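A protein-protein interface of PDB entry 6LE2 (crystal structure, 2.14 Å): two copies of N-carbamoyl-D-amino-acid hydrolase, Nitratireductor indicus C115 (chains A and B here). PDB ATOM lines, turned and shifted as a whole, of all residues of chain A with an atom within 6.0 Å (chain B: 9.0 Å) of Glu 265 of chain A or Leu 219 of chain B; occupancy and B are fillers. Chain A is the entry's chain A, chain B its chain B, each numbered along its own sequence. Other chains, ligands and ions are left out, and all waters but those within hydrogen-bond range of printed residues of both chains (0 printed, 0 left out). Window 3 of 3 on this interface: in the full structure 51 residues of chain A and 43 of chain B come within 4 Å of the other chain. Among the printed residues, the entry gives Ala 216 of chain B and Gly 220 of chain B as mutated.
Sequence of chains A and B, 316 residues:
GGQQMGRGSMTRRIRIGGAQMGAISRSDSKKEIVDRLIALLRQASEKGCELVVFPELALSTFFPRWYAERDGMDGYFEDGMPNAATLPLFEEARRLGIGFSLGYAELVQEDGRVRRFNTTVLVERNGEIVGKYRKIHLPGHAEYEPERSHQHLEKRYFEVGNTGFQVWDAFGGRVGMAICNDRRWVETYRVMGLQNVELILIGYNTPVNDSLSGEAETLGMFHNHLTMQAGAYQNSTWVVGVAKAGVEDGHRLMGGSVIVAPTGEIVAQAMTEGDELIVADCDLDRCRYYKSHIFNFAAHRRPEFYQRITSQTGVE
No position is printed for both chains.
The backbone carbonyl oxygen of Gly 264 of chain A sits at hydrogen-bond distance from the side-chain amide nitrogen of Gln 229 of chain A, 3.0 Å away.
OG1 of Thr 263 of chain A sits at hydrogen-bond distance from OE1 of Glu 265 of chain A.
O of Leu 219 of chain B is in hydrogen-bond range of ND1 of His 223 of chain B (3.3 Å).
OG1 of Thr 227 of chain B lies within hydrogen-bond range of O of His 223 of chain B, at 3.2 Å.
Of the printed residues of chain B, Gln 229 of chain A touches Phe 222 and Leu 226.
No residue of chain B comes within 4 Å of Val 260 of chain A.
No residue of chain B comes within 4 Å of Ala 261 of chain A.
Of chain B, only Phe 222 and His 223 come within 4 Å of Thr 263 of chain A.
Gly 264 of chain A touches one residue of chain B.
Glu 265 of chain A touches one residue of chain B.
Printed residues of chain B within 4 Å of Tyr 290 of chain A: Leu 219 and His 223.
Val 208 of chain B touches none of the printed residues of chain A.
Glu 217 of chain B touches none of the printed residues of chain A.
Of the printed residues of chain A, Leu 219 of chain B touches Glu 265 and Tyr 290.
Of the printed residues of chain A, Phe 222 of chain B touches Gln 229 (3.9 Å), Thr 263 (3.6 Å) and Gly 264 (3.6 Å).
Of the printed residues of chain A, His 223 of chain B touches Thr 263 and Tyr 290.
Of the printed residues of chain A, Leu 226 of chain B touches Gln 229 (3.8 Å).
The nearest residue of chain B that does not touch Glu 265 of chain A is Phe 222 of chain B (4.3 Å).
The nearest residue of chain A that does not touch Leu 219 of chain B is Thr 263 of chain A (4.6 Å).
The nearest printed residue of chain A that does not touch His 223 of chain B is Gly 264 of chain A (4.9 Å).
Hydrophobic or aromatic side chains of chain B within 4 Å of the printed part of chain A: Leu 219, Phe 222, His 223 and Leu 226.
Of the 13 printed residues of chain A, 5 touch a printed residue of chain B.
Printed residues of chain A that touch a printed residue of chain B: Gln 229, Thr 263, Gly 264, Glu 265 and Tyr 290.
Hydrophobic or aromatic side chains of chain A that line the printed part of chain B: Tyr 290.
Among the printed residues, 8 pairs touch across the chains.
O of Thr 263 of chain A is in hydrogen-bond range of NE2 of His 223 of chain B (2.7 Å).
CZ of Phe 222 of chain B touches NE2 of Gln 229 of chain A, 3.9 Å away.
Leu 226 of chain B touches Gln 229 of chain A.
Phe 222 of chain B touches Thr 263 of chain A (CE2 to O, 3.6 Å).
Gly 264 of chain A touches Phe 222 of chain B.
Leu 219 of chain B touches Glu 265 of chain A (CD1 to OE2, 3.5 Å).
OH of Tyr 290 of chain A touches CD2 of Leu 219 of chain B (3.6 Å).
OH of Tyr 290 of chain A touches CE1 of His 223 of chain B, at 3.0 Å.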
ATOM      1  N   GLN A 229      -5.875 -28.155  21.968  1.00  0.00           N
ATOM      2  CA  GLN A 229      -5.968 -26.911  21.220  1.00  0.00           C
ATOM      3  C   GLN A 229      -7.395 -26.654  20.761  1.00  0.00           C
ATOM      4  O   GLN A 229      -7.908 -25.535  20.885  1.00  0.00           O
ATOM      5  CB  GLN A 229      -5.006 -26.948  20.040  1.00  0.00           C
ATOM      6  CG  GLN A 229      -3.566 -26.834  20.480  1.00  0.00           C
ATOM      7  CD  GLN A 229      -2.594 -26.885  19.322  1.00  0.00           C
ATOM      8  OE1 GLN A 229      -2.234 -27.962  18.855  1.00  0.00           O
ATOM      9  NE2 GLN A 229      -2.165 -25.708  18.851  1.00  0.00           N
ATOM     10  N   ILE A 259       0.726 -25.311  27.653  1.00  0.00           N
ATOM     11  CA  ILE A 259      -0.277 -24.344  28.075  1.00  0.00           C
ATOM     12  C   ILE A 259      -0.846 -23.733  26.801  1.00  0.00           C
ATOM     13  O   ILE A 259      -0.088 -23.277  25.939  1.00  0.00           O
ATOM     14  CB  ILE A 259       0.315 -23.260  28.999  1.00  0.00           C
ATOM     15  CG1 ILE A 259       0.824 -23.895  30.307  1.00  0.00           C
ATOM     16  CG2 ILE A 259      -0.729 -22.183  29.294  1.00  0.00           C
ATOM     17  CD1 ILE A 259       1.706 -22.933  31.216  1.00  0.00           C
ATOM     18  N   VAL A 260      -2.168 -23.740  26.678  1.00  0.00           N
ATOM     19  CA  VAL A 260      -2.859 -23.389  25.441  1.00  0.00           C
ATOM     20  C   VAL A 260      -3.776 -22.211  25.718  1.00  0.00           C
ATOM     21  O   VAL A 260      -4.535 -22.236  26.690  1.00  0.00           O
ATOM     22  CB  VAL A 260      -3.678 -24.574  24.906  1.00  0.00           C
ATOM     23  CG1 VAL A 260      -4.335 -24.207  23.586  1.00  0.00           C
ATOM     24  CG2 VAL A 260      -2.797 -25.798  24.785  1.00  0.00           C
ATOM     25  N   ALA A 261      -3.722 -21.199  24.854  1.00  0.00           N
ATOM     26  CA  ALA A 261      -4.526 -19.995  25.006  1.00  0.00           C
ATOM     27  C   ALA A 261      -5.936 -20.222  24.454  1.00  0.00           C
ATOM     28  O   ALA A 261      -6.162 -21.147  23.672  1.00  0.00           O
ATOM     29  CB  ALA A 261      -3.844 -18.832  24.278  1.00  0.00           C
ATOM     30  N   PRO A 262      -6.908 -19.389  24.846  1.00  0.00           N
ATOM     31  CA  PRO A 262      -8.279 -19.560  24.320  1.00  0.00           C
ATOM     32  C   PRO A 262      -8.382 -19.393  22.815  1.00  0.00           C
ATOM     33  O   PRO A 262      -9.446 -19.685  22.249  1.00  0.00           O
ATOM     34  CB  PRO A 262      -9.080 -18.475  25.056  1.00  0.00           C
ATOM     35  CG  PRO A 262      -8.053 -17.499  25.526  1.00  0.00           C
ATOM     36  CD  PRO A 262      -6.861 -18.336  25.872  1.00  0.00           C
ATOM     37  N   THR A 263      -7.324 -18.921  22.161  1.00  0.00           N
ATOM     38  CA  THR A 263      -7.226 -18.952  20.715  1.00  0.00           C
ATOM     39  C   THR A 263      -6.869 -20.330  20.184  1.00  0.00           C
ATOM     40  O   THR A 263      -6.859 -20.521  18.961  1.00  0.00           O
ATOM     41  CB  THR A 263      -6.152 -17.988  20.243  1.00  0.00           C
ATOM     42  OG1 THR A 263      -4.892 -18.444  20.742  1.00  0.00           O
ATOM     43  CG2 THR A 263      -6.419 -16.593  20.753  1.00  0.00           C
ATOM     44  N   GLY A 264      -6.541 -21.275  21.063  1.00  0.00           N
ATOM     45  CA  GLY A 264      -6.037 -22.555  20.621  1.00  0.00           C
ATOM     46  C   GLY A 264      -4.550 -22.588  20.350  1.00  0.00           C
ATOM     47  O   GLY A 264      -4.034 -23.641  19.971  1.00  0.00           O
ATOM     48  N   GLU A 265      -3.840 -21.482  20.545  1.00  0.00           N
ATOM     49  CA  GLU A 265      -2.401 -21.477  20.327  1.00  0.00           C
ATOM     50  C   GLU A 265      -1.668 -21.973  21.563  1.00  0.00           C
ATOM     51  O   GLU A 265      -2.039 -21.652  22.693  1.00  0.00           O
ATOM     52  CB  GLU A 265      -1.911 -20.075  19.984  1.00  0.00           C
ATOM     53  CG  GLU A 265      -2.416 -19.521  18.680  1.00  0.00           C
ATOM     54  CD  GLU A 265      -2.203 -18.015  18.608  1.00  0.00           C
ATOM     55  OE1 GLU A 265      -2.786 -17.283  19.453  1.00  0.00           O
ATOM     56  OE2 GLU A 265      -1.431 -17.577  17.735  1.00  0.00           O
ATOM     57  N   ILE A 266      -0.638 -22.777  21.336  1.00  0.00           N
ATOM     58  CA  ILE A 266       0.277 -23.204  22.389  1.00  0.00           C
ATOM     59  C   ILE A 266       1.172 -22.021  22.741  1.00  0.00           C
ATOM     60  O   ILE A 266       1.836 -21.459  21.868  1.00  0.00           O
ATOM     61  CB  ILE A 266       1.110 -24.417  21.931  1.00  0.00           C
ATOM     62  CG1 ILE A 266       0.214 -25.642  21.726  1.00  0.00           C
ATOM     63  CG2 ILE A 266       2.203 -24.737  22.944  1.00  0.00           C
ATOM     64  CD1 ILE A 266       0.899 -26.835  21.114  1.00  0.00           C
ATOM     65  N   VAL A 267       1.185 -21.634  24.017  1.00  0.00           N
ATOM     66  CA  VAL A 267       2.063 -20.566  24.485  1.00  0.00           C
ATOM     67  C   VAL A 267       3.237 -21.083  25.298  1.00  0.00           C
ATOM     68  O   VAL A 267       4.118 -20.288  25.652  1.00  0.00           O
ATOM     69  CB  VAL A 267       1.285 -19.508  25.300  1.00  0.00           C
ATOM     70  CG1 VAL A 267       0.286 -18.806  24.418  1.00  0.00           C
ATOM     71  CG2 VAL A 267       0.577 -20.154  26.478  1.00  0.00           C
ATOM     72  N   ARG A 286      -8.714 -12.545  28.391  1.00  0.00           N
ATOM     73  CA  ARG A 286      -8.614 -12.914  26.991  1.00  0.00           C
ATOM     74  C   ARG A 286      -9.703 -13.907  26.608  1.00  0.00           C
ATOM     75  O   ARG A 286     -10.005 -14.042  25.420  1.00  0.00           O
ATOM     76  CB  ARG A 286      -7.229 -13.499  26.700  1.00  0.00           C
ATOM     77  CG  ARG A 286      -6.963 -13.734  25.236  1.00  0.00           C
ATOM     78  CD  ARG A 286      -5.695 -13.042  24.805  1.00  0.00           C
ATOM     79  NE  ARG A 286      -4.540 -13.902  25.036  1.00  0.00           N
ATOM     80  CZ  ARG A 286      -3.866 -14.525  24.074  1.00  0.00           C
ATOM     81  NH1 ARG A 286      -2.828 -15.288  24.381  1.00  0.00           N
ATOM     82  NH2 ARG A 286      -4.215 -14.363  22.802  1.00  0.00           N
ATOM     83  N   TYR A 289     -12.455 -12.836  24.348  1.00  0.00           N
ATOM     84  CA  TYR A 289     -12.129 -12.699  22.930  1.00  0.00           C
ATOM     85  C   TYR A 289     -13.177 -13.369  22.040  1.00  0.00           C
ATOM     86  O   TYR A 289     -13.696 -12.756  21.101  1.00  0.00           O
ATOM     87  CB  TYR A 289     -10.741 -13.300  22.682  1.00  0.00           C
ATOM     88  CG  TYR A 289      -9.949 -12.771  21.505  1.00  0.00           C
ATOM     89  CD1 TYR A 289      -8.554 -12.793  21.529  1.00  0.00           C
ATOM     90  CD2 TYR A 289     -10.580 -12.279  20.366  1.00  0.00           C
ATOM     91  CE1 TYR A 289      -7.811 -12.324  20.462  1.00  0.00           C
ATOM     92  CE2 TYR A 289      -9.846 -11.809  19.289  1.00  0.00           C
ATOM     93  CZ  TYR A 289      -8.462 -11.833  19.344  1.00  0.00           C
ATOM     94  OH  TYR A 289      -7.730 -11.363  18.275  1.00  0.00           O
ATOM     95  N   TYR A 290     -13.492 -14.641  22.317  1.00  0.00           N
ATOM     96  CA  TYR A 290     -14.479 -15.364  21.523  1.00  0.00           C
ATOM     97  C   TYR A 290     -15.814 -15.584  22.231  1.00  0.00           C
ATOM     98  O   TYR A 290     -16.809 -15.860  21.550  1.00  0.00           O
ATOM     99  CB  TYR A 290     -13.899 -16.714  21.053  1.00  0.00           C
ATOM    100  CG  TYR A 290     -12.649 -16.539  20.206  1.00  0.00           C
ATOM    101  CD1 TYR A 290     -12.725 -15.971  18.939  1.00  0.00           C
ATOM    102  CD2 TYR A 290     -11.390 -16.909  20.686  1.00  0.00           C
ATOM    103  CE1 TYR A 290     -11.581 -15.776  18.161  1.00  0.00           C
ATOM    104  CE2 TYR A 290     -10.239 -16.717  19.916  1.00  0.00           C
ATOM    105  CZ  TYR A 290     -10.342 -16.147  18.656  1.00  0.00           C
ATOM    106  OH  TYR A 290      -9.223 -15.943  17.874  1.00  0.00           O
ATOM    107  N   VAL B 208     -13.194 -12.897   5.434  1.00  0.00           N
ATOM    108  CA  VAL B 208     -11.902 -12.584   6.032  1.00  0.00           C
ATOM    109  C   VAL B 208     -11.883 -11.100   6.362  1.00  0.00           C
ATOM    110  O   VAL B 208     -12.294 -10.264   5.546  1.00  0.00           O
ATOM    111  CB  VAL B 208     -10.749 -12.967   5.089  1.00  0.00           C
ATOM    112  CG1 VAL B 208      -9.428 -12.380   5.574  1.00  0.00           C
ATOM    113  CG2 VAL B 208     -10.651 -14.475   5.002  1.00  0.00           C
ATOM    114  N   GLU B 215      -1.147 -12.434   9.542  1.00  0.00           N
ATOM    115  CA  GLU B 215      -1.879 -11.567  10.454  1.00  0.00           C
ATOM    116  C   GLU B 215      -2.928 -12.346  11.247  1.00  0.00           C
ATOM    117  O   GLU B 215      -2.696 -13.475  11.684  1.00  0.00           O
ATOM    118  CB  GLU B 215      -2.564 -10.441   9.678  1.00  0.00           C
ATOM    119  CG  GLU B 215      -1.687  -9.744   8.664  1.00  0.00           C
ATOM    120  CD  GLU B 215      -0.827  -8.667   9.288  1.00  0.00           C
ATOM    121  OE1 GLU B 215      -0.395  -7.751   8.553  1.00  0.00           O
ATOM    122  OE2 GLU B 215      -0.592  -8.726  10.513  1.00  0.00           O
ATOM    123  N   ALA B 216      -4.084 -11.711  11.444  1.00  0.00           N
ATOM    124  CA  ALA B 216      -5.283 -12.411  11.884  1.00  0.00           C
ATOM    125  C   ALA B 216      -5.913 -13.232  10.767  1.00  0.00           C
ATOM    126  O   ALA B 216      -6.871 -13.969  11.025  1.00  0.00           O
ATOM    127  CB  ALA B 216      -6.303 -11.412  12.430  1.00  0.00           C
ATOM    128  N   GLU B 217      -5.417 -13.092   9.531  1.00  0.00           N
ATOM    129  CA  GLU B 217      -5.812 -13.999   8.459  1.00  0.00           C
ATOM    130  C   GLU B 217      -5.243 -15.388   8.698  1.00  0.00           C
ATOM    131  O   GLU B 217      -5.919 -16.394   8.454  1.00  0.00           O
ATOM    132  CB  GLU B 217      -5.341 -13.474   7.100  1.00  0.00           C
ATOM    133  CG  GLU B 217      -5.956 -12.155   6.655  1.00  0.00           C
ATOM    134  CD  GLU B 217      -5.363 -10.954   7.373  1.00  0.00           C
ATOM    135  OE1 GLU B 217      -5.883 -10.586   8.449  1.00  0.00           O
ATOM    136  OE2 GLU B 217      -4.369 -10.386   6.867  1.00  0.00           O
ATOM    137  N   THR B 218      -3.993 -15.456   9.165  1.00  0.00           N
ATOM    138  CA  THR B 218      -3.374 -16.738   9.472  1.00  0.00           C
ATOM    139  C   THR B 218      -4.071 -17.419  10.644  1.00  0.00           C
ATOM    140  O   THR B 218      -4.195 -18.647  10.668  1.00  0.00           O
ATOM    141  CB  THR B 218      -1.890 -16.539   9.766  1.00  0.00           C
ATOM    142  OG1 THR B 218      -1.740 -15.483  10.720  1.00  0.00           O
ATOM    143  CG2 THR B 218      -1.130 -16.179   8.484  1.00  0.00           C
ATOM    144  N   LEU B 219      -4.546 -16.637  11.618  1.00  0.00           N
ATOM    145  CA  LEU B 219      -5.266 -17.217  12.746  1.00  0.00           C
ATOM    146  C   LEU B 219      -6.640 -17.725  12.318  1.00  0.00           C
ATOM    147  O   LEU B 219      -7.086 -18.793  12.763  1.00  0.00           O
ATOM    148  CB  LEU B 219      -5.394 -16.186  13.863  1.00  0.00           C
ATOM    149  CG  LEU B 219      -5.619 -16.748  15.267  1.00  0.00           C
ATOM    150  CD1 LEU B 219      -4.380 -17.484  15.770  1.00  0.00           C
ATOM    151  CD2 LEU B 219      -6.022 -15.640  16.221  1.00  0.00           C
ATOM    152  N   GLY B 220      -7.325 -16.962  11.461  1.00  0.00           N
ATOM    153  CA  GLY B 220      -8.539 -17.456  10.836  1.00  0.00           C
ATOM    154  C   GLY B 220      -8.332 -18.780  10.125  1.00  0.00           C
ATOM    155  O   GLY B 220      -9.134 -19.707  10.274  1.00  0.00           O
ATOM    156  N   MET B 221      -7.249 -18.893   9.352  1.00  0.00           N
ATOM    157  CA  MET B 221      -6.978 -20.148   8.649  1.00  0.00           C
ATOM    158  C   MET B 221      -6.671 -21.265   9.641  1.00  0.00           C
ATOM    159  O   MET B 221      -7.178 -22.383   9.508  1.00  0.00           O
ATOM    160  CB  MET B 221      -5.826 -19.965   7.657  1.00  0.00           C
ATOM    161  CG  MET B 221      -5.612 -21.150   6.714  1.00  0.00           C
ATOM    162  SD  MET B 221      -7.093 -21.557   5.747  1.00  0.00           S
ATOM    163  CE  MET B 221      -7.031 -20.218   4.529  1.00  0.00           C
ATOM    164  N   PHE B 222      -5.873 -20.961  10.661  1.00  0.00           N
ATOM    165  CA  PHE B 222      -5.609 -21.908  11.739  1.00  0.00           C
ATOM    166  C   PHE B 222      -6.909 -22.438  12.353  1.00  0.00           C
ATOM    167  O   PHE B 222      -7.092 -23.653  12.494  1.00  0.00           O
ATOM    168  CB  PHE B 222      -4.724 -21.225  12.792  1.00  0.00           C
ATOM    169  CG  PHE B 222      -4.556 -22.017  14.055  1.00  0.00           C
ATOM    170  CD1 PHE B 222      -3.855 -23.210  14.056  1.00  0.00           C
ATOM    171  CD2 PHE B 222      -5.092 -21.562  15.242  1.00  0.00           C
ATOM    172  CE1 PHE B 222      -3.708 -23.932  15.220  1.00  0.00           C
ATOM    173  CE2 PHE B 222      -4.946 -22.279  16.415  1.00  0.00           C
ATOM    174  CZ  PHE B 222      -4.254 -23.466  16.405  1.00  0.00           C
ATOM    175  N   HIS B 223      -7.838 -21.540  12.696  1.00  0.00           N
ATOM    176  CA  HIS B 223      -9.107 -21.968  13.286  1.00  0.00           C
ATOM    177  C   HIS B 223      -9.952 -22.772  12.306  1.00  0.00           C
ATOM    178  O   HIS B 223     -10.594 -23.752  12.700  1.00  0.00           O
ATOM    179  CB  HIS B 223      -9.886 -20.760  13.793  1.00  0.00           C
ATOM    180  CG  HIS B 223      -9.220 -20.073  14.938  1.00  0.00           C
ATOM    181  ND1 HIS B 223      -9.333 -18.721  15.175  1.00  0.00           N
ATOM    182  CD2 HIS B 223      -8.424 -20.564  15.915  1.00  0.00           C
ATOM    183  CE1 HIS B 223      -8.632 -18.407  16.248  1.00  0.00           C
ATOM    184  NE2 HIS B 223      -8.069 -19.509  16.715  1.00  0.00           N
ATOM    185  N   ASN B 224      -9.976 -22.361  11.034  1.00  0.00           N
ATOM    186  CA  ASN B 224     -10.649 -23.131   9.984  1.00  0.00           C
ATOM    187  C   ASN B 224     -10.200 -24.593   9.989  1.00  0.00           C
ATOM    188  O   ASN B 224     -11.023 -25.513  10.067  1.00  0.00           O
ATOM    189  CB  ASN B 224     -10.367 -22.473   8.627  1.00  0.00           C
ATOM    190  CG  ASN B 224     -11.045 -23.176   7.475  1.00  0.00           C
ATOM    191  OD1 ASN B 224     -12.168 -23.673   7.607  1.00  0.00           O
ATOM    192  ND2 ASN B 224     -10.370 -23.206   6.317  1.00  0.00           N
ATOM    193  N   HIS B 225      -8.889 -24.829   9.929  1.00  0.00           N
ATOM    194  CA  HIS B 225      -8.415 -26.205   9.897  1.00  0.00           C
ATOM    195  C   HIS B 225      -8.523 -26.869  11.262  1.00  0.00           C
ATOM    196  O   HIS B 225      -8.863 -28.054  11.346  1.00  0.00           O
ATOM    197  CB  HIS B 225      -6.980 -26.253   9.372  1.00  0.00           C
ATOM    198  CG  HIS B 225      -6.865 -25.793   7.957  1.00  0.00           C
ATOM    199  ND1 HIS B 225      -5.661 -25.482   7.359  1.00  0.00           N
ATOM    200  CD2 HIS B 225      -7.820 -25.588   7.019  1.00  0.00           C
ATOM    201  CE1 HIS B 225      -5.882 -25.108   6.110  1.00  0.00           C
ATOM    202  NE2 HIS B 225      -7.184 -25.156   5.883  1.00  0.00           N
ATOM    203  N   LEU B 226      -8.260 -26.122  12.341  1.00  0.00           N
ATOM    204  CA  LEU B 226      -8.277 -26.719  13.673  1.00  0.00           C
ATOM    205  C   LEU B 226      -9.625 -27.370  13.965  1.00  0.00           C
ATOM    206  O   LEU B 226      -9.686 -28.503  14.456  1.00  0.00           O
ATOM    207  CB  LEU B 226      -7.948 -25.661  14.735  1.00  0.00           C
ATOM    208  CG  LEU B 226      -8.029 -26.088  16.212  1.00  0.00           C
ATOM    209  CD1 LEU B 226      -6.909 -27.075  16.547  1.00  0.00           C
ATOM    210  CD2 LEU B 226      -7.994 -24.851  17.174  1.00  0.00           C
ATOM    211  N   THR B 227     -10.723 -26.671  13.666  1.00  0.00           N
ATOM    212  CA  THR B 227     -12.031 -27.213  14.021  1.00  0.00           C
ATOM    213  C   THR B 227     -12.363 -28.451  13.190  1.00  0.00           C
ATOM    214  O   THR B 227     -12.921 -29.418  13.712  1.00  0.00           O
ATOM    215  CB  THR B 227     -13.114 -26.152  13.855  1.00  0.00           C
ATOM    216  OG1 THR B 227     -13.095 -25.662  12.512  1.00  0.00           O
ATOM    217  CG2 THR B 227     -12.881 -24.976  14.818  1.00  0.00           C
ATOM    218  N   MET B 254     -12.451 -16.526   2.580  1.00  0.00           N
ATOM    219  CA  MET B 254     -11.328 -17.388   2.929  1.00  0.00           C
ATOM    220  C   MET B 254     -11.203 -18.569   1.972  1.00  0.00           C
ATOM    221  O   MET B 254     -12.206 -19.136   1.529  1.00  0.00           O
ATOM    222  CB  MET B 254     -11.526 -17.905   4.354  1.00  0.00           C
ATOM    223  CG  MET B 254     -10.466 -18.830   4.882  1.00  0.00           C
ATOM    224  SD  MET B 254     -10.909 -19.420   6.534  1.00  0.00           S
ATOM    225  CE  MET B 254     -10.600 -17.967   7.548  1.00  0.00           C
